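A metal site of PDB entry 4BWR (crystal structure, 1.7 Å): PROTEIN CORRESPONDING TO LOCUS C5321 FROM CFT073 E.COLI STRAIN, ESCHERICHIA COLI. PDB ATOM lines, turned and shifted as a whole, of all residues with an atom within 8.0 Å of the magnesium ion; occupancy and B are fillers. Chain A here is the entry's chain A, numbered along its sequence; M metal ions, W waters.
OE2 of Glu 100 is in hydrogen-bond range of ND1 of His 99 (2.8 Å).
OD1 of Asp 138 lies within salt-bridge range of NZ of Lys 108 (2.9 Å).
The backbone NH of Asp 138 lies within hydrogen-bond range of the backbone carbonyl oxygen of Ala 133, at 2.9 Å.
Of the 14 residues printed, 3 come within 4 Å of the magnesium ion.
The nearest printed residue that does not touch the magnesium ion is Lys 108 (4.4 Å).
The magnesium ion is bound by the side-chain carboxylate (OD2) of Asp 138 (2.0 Å), water W1 (2.1 Å), the side-chain carboxylate (OE1) of Glu 136 (2.2 Å), water W3 (2.2 Å), water W2 (2.2 Å) and a ring nitrogen (NE2) of His 99 (2.2 Å).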
ATOM      1  N   HIS A  99      24.779  -0.476 -12.961  1.00  0.00           N
ATOM      2  CA  HIS A  99      23.708  -1.341 -12.467  1.00  0.00           C
ATOM      3  C   HIS A  99      22.456  -0.518 -12.159  1.00  0.00           C
ATOM      4  O   HIS A  99      21.327  -0.973 -12.421  1.00  0.00           O
ATOM      5  CB  HIS A  99      24.184  -2.095 -11.213  1.00  0.00           C
ATOM      6  CG  HIS A  99      23.164  -3.039 -10.649  1.00  0.00           C
ATOM      7  ND1 HIS A  99      22.142  -2.623  -9.821  1.00  0.00           N
ATOM      8  CD2 HIS A  99      23.020  -4.380 -10.781  1.00  0.00           C
ATOM      9  CE1 HIS A  99      21.401  -3.665  -9.472  1.00  0.00           C
ATOM     10  NE2 HIS A  99      21.914  -4.740 -10.043  1.00  0.00           N
ATOM     11  N   GLU A 100      22.673   0.688 -11.644  1.00  0.00           N
ATOM     12  CA  GLU A 100      21.596   1.582 -11.211  1.00  0.00           C
ATOM     13  C   GLU A 100      21.131   2.541 -12.307  1.00  0.00           C
ATOM     14  O   GLU A 100      20.078   3.160 -12.188  1.00  0.00           O
ATOM     15  CB  GLU A 100      22.059   2.408 -10.010  1.00  0.00           C
ATOM     16  CG  GLU A 100      22.376   1.583  -8.772  1.00  0.00           C
ATOM     17  CD  GLU A 100      21.157   0.810  -8.266  1.00  0.00           C
ATOM     18  OE1 GLU A 100      20.241   1.443  -7.702  1.00  0.00           O
ATOM     19  OE2 GLU A 100      21.106  -0.421  -8.456  1.00  0.00           O
ATOM     20  N   LYS A 108      23.271  -3.831 -17.447  1.00  0.00           N
ATOM     21  CA  LYS A 108      23.575  -4.853 -16.452  1.00  0.00           C
ATOM     22  C   LYS A 108      24.779  -5.698 -16.853  1.00  0.00           C
ATOM     23  O   LYS A 108      25.591  -6.052 -16.002  1.00  0.00           O
ATOM     24  CB  LYS A 108      22.346  -5.730 -16.201  1.00  0.00           C
ATOM     25  CG  LYS A 108      21.204  -4.976 -15.549  1.00  0.00           C
ATOM     26  CD  LYS A 108      21.561  -4.515 -14.140  1.00  0.00           C
ATOM     27  CE  LYS A 108      20.391  -3.868 -13.424  1.00  0.00           C
ATOM     28  NZ  LYS A 108      19.289  -4.839 -13.174  1.00  0.00           N
ATOM     29  N   SER A 111      27.724  -3.694 -15.987  1.00  0.00           N
ATOM     30  CA  SER A 111      27.958  -3.664 -14.541  1.00  0.00           C
ATOM     31  C   SER A 111      28.781  -4.884 -14.139  1.00  0.00           C
ATOM     32  O   SER A 111      29.724  -4.776 -13.354  1.00  0.00           O
ATOM     33  CB  SER A 111      26.646  -3.606 -13.748  1.00  0.00           C
ATOM     34  OG  SER A 111      25.943  -4.851 -13.760  1.00  0.00           O
ATOM     35  N   VAL A 112      28.438  -6.037 -14.717  1.00  0.00           N
ATOM     36  CA  VAL A 112      29.127  -7.274 -14.386  1.00  0.00           C
ATOM     37  C   VAL A 112      30.600  -7.226 -14.816  1.00  0.00           C
ATOM     38  O   VAL A 112      31.466  -7.714 -14.096  1.00  0.00           O
ATOM     39  CB  VAL A 112      28.411  -8.510 -14.977  1.00  0.00           C
ATOM     40  CG1 VAL A 112      29.230  -9.788 -14.788  1.00  0.00           C
ATOM     41  CG2 VAL A 112      27.042  -8.677 -14.335  1.00  0.00           C
ATOM     42  N   PHE A 115      32.223  -5.186 -11.953  1.00  0.00           N
ATOM     43  CA  PHE A 115      32.231  -5.944 -10.700  1.00  0.00           C
ATOM     44  C   PHE A 115      33.257  -7.073 -10.760  1.00  0.00           C
ATOM     45  O   PHE A 115      33.940  -7.356  -9.776  1.00  0.00           O
ATOM     46  CB  PHE A 115      30.865  -6.570 -10.432  1.00  0.00           C
ATOM     47  CG  PHE A 115      29.763  -5.592 -10.135  1.00  0.00           C
ATOM     48  CD1 PHE A 115      29.983  -4.464  -9.390  1.00  0.00           C
ATOM     49  CD2 PHE A 115      28.476  -5.841 -10.597  1.00  0.00           C
ATOM     50  CE1 PHE A 115      28.964  -3.576  -9.120  1.00  0.00           C
ATOM     51  CE2 PHE A 115      27.460  -4.967 -10.332  1.00  0.00           C
ATOM     52  CZ  PHE A 115      27.701  -3.840  -9.591  1.00  0.00           C
ATOM     53  N   SER A 129      28.951  -8.623  -5.257  1.00  0.00           N
ATOM     54  CA  SER A 129      28.225  -8.169  -6.436  1.00  0.00           C
ATOM     55  C   SER A 129      28.147  -9.256  -7.495  1.00  0.00           C
ATOM     56  O   SER A 129      27.129  -9.414  -8.173  1.00  0.00           O
ATOM     57  CB  SER A 129      28.859  -6.885  -7.006  1.00  0.00           C
ATOM     58  OG  SER A 129      28.559  -5.787  -6.159  1.00  0.00           O
ATOM     59  N   ASP A 132      25.564 -11.808  -6.264  1.00  0.00           N
ATOM     60  CA  ASP A 132      24.219 -11.291  -6.505  1.00  0.00           C
ATOM     61  C   ASP A 132      23.865 -11.371  -7.995  1.00  0.00           C
ATOM     62  O   ASP A 132      22.744 -11.730  -8.357  1.00  0.00           O
ATOM     63  CB  ASP A 132      24.079  -9.851  -6.014  1.00  0.00           C
ATOM     64  CG  ASP A 132      24.129  -9.725  -4.495  1.00  0.00           C
ATOM     65  OD1 ASP A 132      23.804 -10.714  -3.799  1.00  0.00           O
ATOM     66  OD2 ASP A 132      24.470  -8.639  -3.980  1.00  0.00           O
ATOM     67  N   ALA A 133      24.815 -11.030  -8.859  1.00  0.00           N
ATOM     68  CA  ALA A 133      24.571 -11.083 -10.292  1.00  0.00           C
ATOM     69  C   ALA A 133      24.186 -12.493 -10.729  1.00  0.00           C
ATOM     70  O   ALA A 133      23.203 -12.683 -11.459  1.00  0.00           O
ATOM     71  CB  ALA A 133      25.783 -10.606 -11.065  1.00  0.00           C
ATOM     72  N   TYR A 134      24.951 -13.490 -10.286  1.00  0.00           N
ATOM     73  CA  TYR A 134      24.689 -14.866 -10.676  1.00  0.00           C
ATOM     74  C   TYR A 134      23.450 -15.427  -9.972  1.00  0.00           C
ATOM     75  O   TYR A 134      22.780 -16.314 -10.508  1.00  0.00           O
ATOM     76  CB  TYR A 134      25.904 -15.740 -10.375  1.00  0.00           C
ATOM     77  CG  TYR A 134      26.939 -15.724 -11.472  1.00  0.00           C
ATOM     78  CD1 TYR A 134      26.677 -16.295 -12.708  1.00  0.00           C
ATOM     79  CD2 TYR A 134      28.191 -15.158 -11.259  1.00  0.00           C
ATOM     80  CE1 TYR A 134      27.634 -16.280 -13.721  1.00  0.00           C
ATOM     81  CE2 TYR A 134      29.148 -15.147 -12.262  1.00  0.00           C
ATOM     82  CZ  TYR A 134      28.862 -15.703 -13.490  1.00  0.00           C
ATOM     83  OH  TYR A 134      29.812 -15.691 -14.481  1.00  0.00           O
ATOM     84  N   GLU A 136      20.780 -13.586  -9.230  1.00  0.00           N
ATOM     85  CA  GLU A 136      19.646 -12.912  -9.850  1.00  0.00           C
ATOM     86  C   GLU A 136      19.501 -13.245 -11.321  1.00  0.00           C
ATOM     87  O   GLU A 136      18.418 -13.109 -11.893  1.00  0.00           O
ATOM     88  CB  GLU A 136      19.807 -11.401  -9.720  1.00  0.00           C
ATOM     89  CG  GLU A 136      19.760 -10.864  -8.303  1.00  0.00           C
ATOM     90  CD  GLU A 136      20.322  -9.454  -8.213  1.00  0.00           C
ATOM     91  OE1 GLU A 136      20.458  -8.798  -9.274  1.00  0.00           O
ATOM     92  OE2 GLU A 136      20.638  -9.012  -7.084  1.00  0.00           O
ATOM     93  N   GLY A 137      20.597 -13.663 -11.948  1.00  0.00           N
ATOM     94  CA  GLY A 137      20.678 -13.719 -13.392  1.00  0.00           C
ATOM     95  C   GLY A 137      20.630 -12.303 -13.969  1.00  0.00           C
ATOM     96  O   GLY A 137      19.885 -12.034 -14.899  1.00  0.00           O
ATOM     97  N   ASP A 138      21.437 -11.417 -13.391  1.00  0.00           N
ATOM     98  CA  ASP A 138      21.402  -9.989 -13.721  1.00  0.00           C
ATOM     99  C   ASP A 138      22.687  -9.584 -14.445  1.00  0.00           C
ATOM    100  O   ASP A 138      23.714  -9.325 -13.810  1.00  0.00           O
ATOM    101  CB  ASP A 138      21.228  -9.183 -12.423  1.00  0.00           C
ATOM    102  CG  ASP A 138      20.738  -7.780 -12.654  1.00  0.00           C
ATOM    103  OD1 ASP A 138      20.343  -7.468 -13.797  1.00  0.00           O
ATOM    104  OD2 ASP A 138      20.724  -6.992 -11.688  1.00  0.00           O
ATOM    105  N   GLY A 139      22.634  -9.544 -15.778  1.00  0.00           N
ATOM    106  CA  GLY A 139      23.807  -9.232 -16.588  1.00  0.00           C
ATOM    107  C   GLY A 139      24.600 -10.472 -16.930  1.00  0.00           C
ATOM    108  O   GLY A 139      25.580 -10.420 -17.674  1.00  0.00           O
HETATM  109 MG    MG M   1      21.228  -6.854  -9.789  1.00  0.00          MG
HETATM  110  O   HOH W   1      23.190  -7.521 -10.150  1.00  0.00           O
HETATM  111  O   HOH W   2      19.275  -6.052  -9.324  1.00  0.00           O
HETATM  112  O   HOH W   3      21.760  -6.704  -7.701  1.00  0.00           O
